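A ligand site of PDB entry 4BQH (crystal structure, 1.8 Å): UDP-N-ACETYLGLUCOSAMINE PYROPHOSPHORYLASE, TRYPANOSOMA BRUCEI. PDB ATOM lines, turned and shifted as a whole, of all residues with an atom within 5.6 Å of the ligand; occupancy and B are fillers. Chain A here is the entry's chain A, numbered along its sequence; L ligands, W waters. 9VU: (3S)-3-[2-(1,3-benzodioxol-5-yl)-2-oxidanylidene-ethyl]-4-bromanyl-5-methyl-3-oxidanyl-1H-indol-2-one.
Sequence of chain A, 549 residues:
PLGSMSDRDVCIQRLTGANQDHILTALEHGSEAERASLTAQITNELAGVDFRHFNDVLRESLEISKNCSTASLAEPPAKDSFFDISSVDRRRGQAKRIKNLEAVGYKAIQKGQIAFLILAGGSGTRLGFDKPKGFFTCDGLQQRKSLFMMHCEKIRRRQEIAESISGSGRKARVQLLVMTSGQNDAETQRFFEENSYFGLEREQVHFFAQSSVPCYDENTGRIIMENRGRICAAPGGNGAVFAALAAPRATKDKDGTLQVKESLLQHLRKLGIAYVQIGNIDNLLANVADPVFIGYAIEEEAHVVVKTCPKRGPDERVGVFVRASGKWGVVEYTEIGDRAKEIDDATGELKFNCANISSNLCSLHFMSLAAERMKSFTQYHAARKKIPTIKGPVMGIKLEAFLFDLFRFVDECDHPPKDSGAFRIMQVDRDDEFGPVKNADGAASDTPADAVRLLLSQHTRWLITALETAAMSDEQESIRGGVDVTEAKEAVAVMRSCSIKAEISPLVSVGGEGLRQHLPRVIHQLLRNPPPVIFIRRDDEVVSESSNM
Val 49 touches the ligand. His 53 touches the ligand (CD2 to OAL, 3.4 Å). Phe 54 touches the ligand. Ser 211 touches the ligand. Val 213 touches the ligand. O of Gly 236 touches CAX of the ligand, at 3.1 Å. Gly 237 touches the ligand. Gly 239 touches the ligand (C to OAY, 3.7 Å). O of Phe 242 touches CAJ of the ligand (3.9 Å). Ala 243 touches the ligand. Ala 246 touches the ligand (CB to CAJ, 3.8 Å). O of Ala 371 touches CAJ of the ligand, at 3.6 Å. Met 374 touches the ligand (CE to OAY, 3.4 Å). CG of Lys 375 touches CAF of the ligand, at 3.6 Å. Tyr 380 touches the ligand (OH to CAV, 3.3 Å). N of Ala 401 touches CAX of the ligand (3.7 Å). Hydrophobic or aromatic side chains that line the ligand: His 53, Phe 54, Val 213, Ala 240, Ala 243, Ala 246, Ala 371, Met 374, Tyr 380 and Ala 401. 19 residues have an atom within 4 Å of the ligand: Gly 48, Val 49, Asp 50, His 53, Phe 54, Ser 211, Val 213, Gly 236, Gly 237, Gly 239, Ala 240, Phe 242, Ala 243, Ala 246, Ala 371, Met 374, Lys 375, Tyr 380 and Ala 401. The nearest printed residue that does not touch the ligand is Ser 212 (4.5 Å).
The backbone carbonyl oxygen (O) of Gly 48 is in hydrogen-bond range of a nitrogen (NAG) of the ligand, 2.8 Å away. N of Asp 50 is in hydrogen-bond range of OAN of the ligand, at 2.8 Å. The backbone NH (N) of Ala 240 lies close to an oxygen (OAW) of the ligand (3.5 Å).
Water W1 lies within hydrogen-bond range of an oxygen (OAL) of the ligand (2.6 Å) and the backbone carbonyl oxygen of Lys 375 (2.9 Å). Water W3 lies within hydrogen-bond range of OAP of the ligand (2.7 Å) and O of Ala 47 (2.8 Å). Water W4 lies within hydrogen-bond range of NE2 of His 53, O of Met 374, OH of Tyr 380 and OAL of the ligand. Water W2 lies within hydrogen-bond range of the backbone carbonyl oxygen (O) of Gly 239 (2.7 Å), the backbone NH (N) of Ala 243 (2.9 Å) and the side-chain sulfur (SD) of Met 374 (3.3 Å).
The backbone NH (N) of His 53 is in hydrogen-bond range of the side-chain carboxylate (OD1) of Asp 50 (3.1 Å). The backbone NH of Gly 239 sits at hydrogen-bond distance from the backbone carbonyl oxygen of Ala 401 (2.8 Å). The backbone NH (N) of Ala 401 lies within hydrogen-bond range of the backbone carbonyl oxygen (O) of Gly 236, 3.0 Å away. The backbone carbonyl oxygen (O) of Ala 47 is in hydrogen-bond range of the side-chain hydroxyl (OG) of Ser 211, 2.6 Å away.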
ATOM      1  N   ALA A  47      26.295 -31.009  31.337  1.00  0.00           N
ATOM      2  CA  ALA A  47      26.915 -30.393  32.503  1.00  0.00           C
ATOM      3  C   ALA A  47      26.186 -29.090  32.868  1.00  0.00           C
ATOM      4  O   ALA A  47      25.886 -28.273  31.984  1.00  0.00           O
ATOM      5  CB  ALA A  47      28.392 -30.132  32.250  1.00  0.00           C
ATOM      6  N   GLY A  48      25.877 -28.926  34.141  1.00  0.00           N
ATOM      7  CA  GLY A  48      25.311 -27.678  34.638  1.00  0.00           C
ATOM      8  C   GLY A  48      23.821 -27.508  34.431  1.00  0.00           C
ATOM      9  O   GLY A  48      23.221 -26.654  35.092  1.00  0.00           O
ATOM     10  N   VAL A  49      23.203 -28.330  33.559  1.00  0.00           N
ATOM     11  CA  VAL A  49      21.771 -28.227  33.274  1.00  0.00           C
ATOM     12  C   VAL A  49      20.955 -28.452  34.538  1.00  0.00           C
ATOM     13  O   VAL A  49      21.156 -29.443  35.268  1.00  0.00           O
ATOM     14  CB  VAL A  49      21.316 -29.236  32.184  1.00  0.00           C
ATOM     15  CG1 VAL A  49      19.794 -29.398  32.160  1.00  0.00           C
ATOM     16  CG2 VAL A  49      21.890 -28.849  30.812  1.00  0.00           C
ATOM     17  N   ASP A  50      20.029 -27.525  34.795  1.00  0.00           N
ATOM     18  CA  ASP A  50      19.170 -27.578  35.961  1.00  0.00           C
ATOM     19  C   ASP A  50      17.833 -28.183  35.511  1.00  0.00           C
ATOM     20  O   ASP A  50      17.043 -27.531  34.839  1.00  0.00           O
ATOM     21  CB  ASP A  50      19.001 -26.153  36.519  1.00  0.00           C
ATOM     22  CG  ASP A  50      18.118 -26.077  37.767  1.00  0.00           C
ATOM     23  OD1 ASP A  50      17.268 -26.929  38.017  1.00  0.00           O
ATOM     24  OD2 ASP A  50      18.280 -25.074  38.489  1.00  0.00           O
ATOM     25  N   PHE A  51      17.621 -29.461  35.839  1.00  0.00           N
ATOM     26  CA  PHE A  51      16.475 -30.192  35.311  1.00  0.00           C
ATOM     27  C   PHE A  51      15.146 -29.628  35.801  1.00  0.00           C
ATOM     28  O   PHE A  51      14.203 -29.522  35.015  1.00  0.00           O
ATOM     29  CB  PHE A  51      16.622 -31.709  35.575  1.00  0.00           C
ATOM     30  CG  PHE A  51      17.678 -32.348  34.726  1.00  0.00           C
ATOM     31  CD1 PHE A  51      17.392 -32.741  33.410  1.00  0.00           C
ATOM     32  CD2 PHE A  51      18.978 -32.540  35.210  1.00  0.00           C
ATOM     33  CE1 PHE A  51      18.375 -33.295  32.609  1.00  0.00           C
ATOM     34  CE2 PHE A  51      19.962 -33.103  34.413  1.00  0.00           C
ATOM     35  CZ  PHE A  51      19.665 -33.491  33.113  1.00  0.00           C
ATOM     36  N   HIS A  53      14.545 -26.460  36.581  1.00  0.00           N
ATOM     37  CA  HIS A  53      14.410 -25.241  35.801  1.00  0.00           C
ATOM     38  C   HIS A  53      13.889 -25.560  34.422  1.00  0.00           C
ATOM     39  O   HIS A  53      13.017 -24.866  33.905  1.00  0.00           O
ATOM     40  CB  HIS A  53      15.756 -24.498  35.733  1.00  0.00           C
ATOM     41  CG  HIS A  53      15.735 -23.360  34.768  1.00  0.00           C
ATOM     42  ND1 HIS A  53      14.917 -22.289  34.916  1.00  0.00           N
ATOM     43  CD2 HIS A  53      16.456 -23.154  33.595  1.00  0.00           C
ATOM     44  CE1 HIS A  53      15.111 -21.445  33.878  1.00  0.00           C
ATOM     45  NE2 HIS A  53      16.058 -21.956  33.090  1.00  0.00           N
ATOM     46  N   PHE A  54      14.397 -26.618  33.798  1.00  0.00           N
ATOM     47  CA  PHE A  54      13.920 -26.940  32.451  1.00  0.00           C
ATOM     48  C   PHE A  54      12.469 -27.404  32.332  1.00  0.00           C
ATOM     49  O   PHE A  54      11.853 -27.248  31.268  1.00  0.00           O
ATOM     50  CB  PHE A  54      14.903 -27.850  31.712  1.00  0.00           C
ATOM     51  CG  PHE A  54      15.924 -27.065  30.923  1.00  0.00           C
ATOM     52  CD1 PHE A  54      15.583 -26.535  29.670  1.00  0.00           C
ATOM     53  CD2 PHE A  54      17.194 -26.804  31.458  1.00  0.00           C
ATOM     54  CE1 PHE A  54      16.510 -25.784  28.938  1.00  0.00           C
ATOM     55  CE2 PHE A  54      18.127 -26.055  30.718  1.00  0.00           C
ATOM     56  CZ  PHE A  54      17.773 -25.535  29.472  1.00  0.00           C
ATOM     57  N   SER A 211      26.528 -27.367  26.696  1.00  0.00           N
ATOM     58  CA  SER A 211      25.584 -28.421  27.068  1.00  0.00           C
ATOM     59  C   SER A 211      24.465 -28.547  26.066  1.00  0.00           C
ATOM     60  O   SER A 211      23.990 -27.569  25.500  1.00  0.00           O
ATOM     61  CB  SER A 211      25.054 -28.159  28.469  1.00  0.00           C
ATOM     62  OG  SER A 211      26.149 -28.303  29.375  1.00  0.00           O
ATOM     63  N   SER A 212      24.019 -29.776  25.847  1.00  0.00           N
ATOM     64  CA  SER A 212      22.826 -30.027  25.071  1.00  0.00           C
ATOM     65  C   SER A 212      21.592 -29.802  25.950  1.00  0.00           C
ATOM     66  O   SER A 212      21.690 -29.595  27.167  1.00  0.00           O
ATOM     67  CB  SER A 212      22.874 -31.442  24.526  1.00  0.00           C
ATOM     68  OG  SER A 212      22.910 -32.378  25.604  1.00  0.00           O
ATOM     69  N   VAL A 213      20.410 -29.821  25.338  1.00  0.00           N
ATOM     70  CA  VAL A 213      19.157 -29.538  26.045  1.00  0.00           C
ATOM     71  C   VAL A 213      18.239 -30.754  25.855  1.00  0.00           C
ATOM     72  O   VAL A 213      18.108 -31.243  24.729  1.00  0.00           O
ATOM     73  CB  VAL A 213      18.491 -28.279  25.459  1.00  0.00           C
ATOM     74  CG1 VAL A 213      17.107 -28.045  26.089  1.00  0.00           C
ATOM     75  CG2 VAL A 213      19.370 -27.056  25.732  1.00  0.00           C
ATOM     76  N   PRO A 235      21.314 -30.032  20.319  1.00  0.00           N
ATOM     77  CA  PRO A 235      22.047 -28.773  20.466  1.00  0.00           C
ATOM     78  C   PRO A 235      21.070 -27.681  20.849  1.00  0.00           C
ATOM     79  O   PRO A 235      19.958 -27.621  20.274  1.00  0.00           O
ATOM     80  CB  PRO A 235      22.594 -28.529  19.045  1.00  0.00           C
ATOM     81  CG  PRO A 235      22.791 -29.905  18.491  1.00  0.00           C
ATOM     82  CD  PRO A 235      21.578 -30.673  19.014  1.00  0.00           C
ATOM     83  N   GLY A 236      21.450 -26.838  21.800  1.00  0.00           N
ATOM     84  CA  GLY A 236      20.511 -25.878  22.327  1.00  0.00           C
ATOM     85  C   GLY A 236      20.369 -24.603  21.524  1.00  0.00           C
ATOM     86  O   GLY A 236      19.502 -23.803  21.824  1.00  0.00           O
ATOM     87  N   GLY A 237      21.245 -24.379  20.531  1.00  0.00           N
ATOM     88  CA  GLY A 237      21.296 -23.061  19.850  1.00  0.00           C
ATOM     89  C   GLY A 237      22.380 -22.217  20.514  1.00  0.00           C
ATOM     90  O   GLY A 237      22.876 -22.573  21.581  1.00  0.00           O
ATOM     91  N   GLY A 239      22.478 -19.645  22.188  1.00  0.00           N
ATOM     92  CA  GLY A 239      22.251 -19.169  23.558  1.00  0.00           C
ATOM     93  C   GLY A 239      22.995 -20.037  24.570  1.00  0.00           C
ATOM     94  O   GLY A 239      23.227 -19.604  25.684  1.00  0.00           O
ATOM     95  N   ALA A 240      23.429 -21.232  24.140  1.00  0.00           N
ATOM     96  CA  ALA A 240      24.270 -22.093  25.003  1.00  0.00           C
ATOM     97  C   ALA A 240      25.579 -21.452  25.497  1.00  0.00           C
ATOM     98  O   ALA A 240      26.205 -21.961  26.439  1.00  0.00           O
ATOM     99  CB  ALA A 240      24.580 -23.433  24.315  1.00  0.00           C
ATOM    100  N   PHE A 242      26.200 -18.816  27.154  1.00  0.00           N
ATOM    101  CA  PHE A 242      26.233 -18.234  28.511  1.00  0.00           C
ATOM    102  C   PHE A 242      26.514 -19.269  29.589  1.00  0.00           C
ATOM    103  O   PHE A 242      27.401 -19.071  30.442  1.00  0.00           O
ATOM    104  CB  PHE A 242      24.955 -17.444  28.789  1.00  0.00           C
ATOM    105  CG  PHE A 242      24.722 -16.355  27.803  1.00  0.00           C
ATOM    106  CD1 PHE A 242      25.560 -15.214  27.784  1.00  0.00           C
ATOM    107  CD2 PHE A 242      23.694 -16.443  26.891  1.00  0.00           C
ATOM    108  CE1 PHE A 242      25.360 -14.214  26.861  1.00  0.00           C
ATOM    109  CE2 PHE A 242      23.477 -15.425  25.964  1.00  0.00           C
ATOM    110  CZ  PHE A 242      24.311 -14.316  25.951  1.00  0.00           C
ATOM    111  N   ALA A 243      25.795 -20.380  29.532  1.00  0.00           N
ATOM    112  CA  ALA A 243      26.025 -21.517  30.429  1.00  0.00           C
ATOM    113  C   ALA A 243      27.408 -22.114  30.241  1.00  0.00           C
ATOM    114  O   ALA A 243      28.103 -22.454  31.228  1.00  0.00           O
ATOM    115  CB  ALA A 243      24.947 -22.583  30.206  1.00  0.00           C
ATOM    116  N   ALA A 246      30.013 -20.167  31.845  1.00  0.00           N
ATOM    117  CA  ALA A 246      29.784 -20.188  33.307  1.00  0.00           C
ATOM    118  C   ALA A 246      30.314 -21.407  34.038  1.00  0.00           C
ATOM    119  O   ALA A 246      30.468 -21.380  35.275  1.00  0.00           O
ATOM    120  CB  ALA A 246      28.277 -20.019  33.607  1.00  0.00           C
ATOM    121  N   ALA A 371      24.342 -14.062  31.426  1.00  0.00           N
ATOM    122  CA  ALA A 371      24.391 -15.422  32.026  1.00  0.00           C
ATOM    123  C   ALA A 371      23.600 -15.485  33.332  1.00  0.00           C
ATOM    124  O   ALA A 371      22.804 -16.411  33.516  1.00  0.00           O
ATOM    125  CB  ALA A 371      25.826 -15.901  32.216  1.00  0.00           C
ATOM    126  N   GLU A 372      23.778 -14.478  34.190  1.00  0.00           N
ATOM    127  CA  GLU A 372      23.021 -14.401  35.452  1.00  0.00           C
ATOM    128  C   GLU A 372      21.528 -14.370  35.172  1.00  0.00           C
ATOM    129  O   GLU A 372      20.766 -15.147  35.763  1.00  0.00           O
ATOM    130  CB  GLU A 372      23.458 -13.188  36.276  1.00  0.00           C
ATOM    131  CG  GLU A 372      23.252 -13.363  37.777  1.00  0.00           C
ATOM    132  CD  GLU A 372      24.258 -12.572  38.630  1.00  0.00           C
ATOM    133  OE1 GLU A 372      24.131 -11.337  38.658  1.00  0.00           O
ATOM    134  OE2 GLU A 372      25.167 -13.182  39.260  1.00  0.00           O
ATOM    135  N   MET A 374      19.990 -15.390  32.526  1.00  0.00           N
ATOM    136  CA  MET A 374      19.496 -16.556  31.811  1.00  0.00           C
ATOM    137  C   MET A 374      19.134 -17.726  32.719  1.00  0.00           C
ATOM    138  O   MET A 374      18.274 -18.513  32.384  1.00  0.00           O
ATOM    139  CB  MET A 374      20.441 -16.989  30.706  1.00  0.00           C
ATOM    140  CG  MET A 374      19.732 -17.814  29.618  1.00  0.00           C
ATOM    141  SD  MET A 374      20.960 -18.332  28.398  1.00  0.00           S
ATOM    142  CE  MET A 374      19.848 -19.188  27.289  1.00  0.00           C
ATOM    143  N   LYS A 375      19.792 -17.824  33.883  1.00  0.00           N
ATOM    144  CA  LYS A 375      19.479 -18.894  34.831  1.00  0.00           C
ATOM    145  C   LYS A 375      18.014 -18.946  35.242  1.00  0.00           C
ATOM    146  O   LYS A 375      17.539 -19.996  35.603  1.00  0.00           O
ATOM    147  CB  LYS A 375      20.378 -18.809  36.070  1.00  0.00           C
ATOM    148  CG  LYS A 375      21.841 -19.046  35.724  1.00  0.00           C
ATOM    149  CD  LYS A 375      22.701 -19.240  36.959  1.00  0.00           C
ATOM    150  CE  LYS A 375      22.641 -20.683  37.445  1.00  0.00           C
ATOM    151  NZ  LYS A 375      23.761 -20.944  38.405  1.00  0.00           N
ATOM    152  N   SER A 376      17.304 -17.815  35.208  1.00  0.00           N
ATOM    153  CA  SER A 376      15.877 -17.832  35.533  1.00  0.00           C
ATOM    154  C   SER A 376      14.991 -17.553  34.329  1.00  0.00           C
ATOM    155  O   SER A 376      13.779 -17.382  34.456  1.00  0.00           O
ATOM    156  CB  SER A 376      15.569 -16.851  36.675  1.00  0.00           C
ATOM    157  OG  SER A 376      15.762 -15.493  36.285  1.00  0.00           O
ATOM    158  N   TYR A 380      12.127 -19.889  25.982  1.00  0.00           N
ATOM    159  CA  TYR A 380      12.842 -20.561  24.903  1.00  0.00           C
ATOM    160  C   TYR A 380      11.922 -20.760  23.711  1.00  0.00           C
ATOM    161  O   TYR A 380      10.697 -20.512  23.792  1.00  0.00           O
ATOM    162  CB  TYR A 380      13.385 -21.928  25.373  1.00  0.00           C
ATOM    163  CG  TYR A 380      14.615 -21.895  26.268  1.00  0.00           C
ATOM    164  CD1 TYR A 380      14.662 -21.118  27.434  1.00  0.00           C
ATOM    165  CD2 TYR A 380      15.724 -22.703  25.977  1.00  0.00           C
ATOM    166  CE1 TYR A 380      15.759 -21.136  28.276  1.00  0.00           C
ATOM    167  CE2 TYR A 380      16.838 -22.704  26.801  1.00  0.00           C
ATOM    168  CZ  TYR A 380      16.854 -21.933  27.960  1.00  0.00           C
ATOM    169  OH  TYR A 380      17.934 -21.948  28.789  1.00  0.00           O
ATOM    170  N   LEU A 399      13.874 -27.632  22.506  1.00  0.00           N
ATOM    171  CA  LEU A 399      13.882 -26.272  23.032  1.00  0.00           C
ATOM    172  C   LEU A 399      15.165 -25.604  22.641  1.00  0.00           C
ATOM    173  O   LEU A 399      16.222 -26.190  22.774  1.00  0.00           O
ATOM    174  CB  LEU A 399      13.792 -26.311  24.560  1.00  0.00           C
ATOM    175  CG  LEU A 399      12.481 -26.878  25.102  1.00  0.00           C
ATOM    176  CD1 LEU A 399      12.640 -27.161  26.591  1.00  0.00           C
ATOM    177  CD2 LEU A 399      11.328 -25.895  24.878  1.00  0.00           C
ATOM    178  N   GLU A 400      15.084 -24.360  22.168  1.00  0.00           N
ATOM    179  CA  GLU A 400      16.312 -23.661  21.766  1.00  0.00           C
ATOM    180  C   GLU A 400      16.327 -22.251  22.332  1.00  0.00           C
ATOM    181  O   GLU A 400      15.282 -21.643  22.541  1.00  0.00           O
ATOM    182  CB  GLU A 400      16.441 -23.601  20.221  1.00  0.00           C
ATOM    183  CG  GLU A 400      16.699 -24.980  19.586  1.00  0.00           C
ATOM    184  CD  GLU A 400      16.768 -24.953  18.060  1.00  0.00           C
ATOM    185  OE1 GLU A 400      16.336 -23.977  17.423  1.00  0.00           O
ATOM    186  OE2 GLU A 400      17.238 -25.959  17.468  1.00  0.00           O
ATOM    187  N   ALA A 401      17.530 -21.732  22.588  1.00  0.00           N
ATOM    188  CA  ALA A 401      17.647 -20.306  22.867  1.00  0.00           C
ATOM    189  C   ALA A 401      18.847 -19.741  22.121  1.00  0.00           C
ATOM    190  O   ALA A 401      19.818 -20.463  21.845  1.00  0.00           O
ATOM    191  CB  ALA A 401      17.755 -20.024  24.371  1.00  0.00           C
HETATM  192  OAN 9VU L   1      19.928 -25.137  33.292  1.00  0.00           O
HETATM  193  CAH 9VU L   1      20.827 -24.281  33.329  1.00  0.00           C
HETATM  194  NAG 9VU L   1      21.918 -24.387  34.093  1.00  0.00           N
HETATM  195  CAC 9VU L   1      22.681 -23.272  33.928  1.00  0.00           C
HETATM  196  CAB 9VU L   1      23.838 -22.960  34.519  1.00  0.00           C
HETATM  197  CAA 9VU L   1      24.508 -21.747  34.282  1.00  0.00           C
HETATM  198  CAF 9VU L   1      23.914 -20.837  33.402  1.00  0.00           C
HETATM  199  CAJ 9VU L   1      24.552 -19.578  33.128  1.00  0.00           C
HETATM  200  CAE 9VU L   1      22.687 -21.215  32.807  1.00  0.00           C
HETATM  201 BRA  9VU L   1      21.946 -19.986  31.558  1.00  0.00          BR
HETATM  202  CAD 9VU L   1      22.086 -22.412  33.061  1.00  0.00           C
HETATM  203  CAI 9VU L   1      20.858 -23.033  32.643  1.00  0.00           C
HETATM  204  OAL 9VU L   1      19.737 -22.292  33.123  1.00  0.00           O
HETATM  205  CAM 9VU L   1      20.632 -23.115  31.108  1.00  0.00           C
HETATM  206  CAO 9VU L   1      21.612 -24.065  30.379  1.00  0.00           C
HETATM  207  OAP 9VU L   1      22.346 -24.777  31.082  1.00  0.00           O
HETATM  208  CAQ 9VU L   1      21.591 -24.094  28.959  1.00  0.00           C
HETATM  209  CAV 9VU L   1      20.955 -23.112  28.189  1.00  0.00           C
HETATM  210  CAU 9VU L   1      20.938 -23.175  26.845  1.00  0.00           C
HETATM  211  OAY 9VU L   1      20.373 -22.297  25.957  1.00  0.00           O
HETATM  212  CAX 9VU L   1      20.296 -23.052  24.725  1.00  0.00           C
HETATM  213  OAW 9VU L   1      21.384 -23.980  24.836  1.00  0.00           O
HETATM  214  CAT 9VU L   1      21.542 -24.161  26.178  1.00  0.00           C
HETATM  215  CAS 9VU L   1      22.184 -25.129  26.847  1.00  0.00           C
HETATM  216  CAR 9VU L   1      22.229 -25.119  28.239  1.00  0.00           C
HETATM  217  O   HOH W   1      19.120 -22.383  35.686  1.00  0.00           O
HETATM  218  O   HOH W   2      23.236 -20.713  28.186  1.00  0.00           O
HETATM  219  O   HOH W   3      24.789 -25.724  31.762  1.00  0.00           O
HETATM  220  O   HOH W   4      17.831 -20.967  31.326  1.00  0.00           O
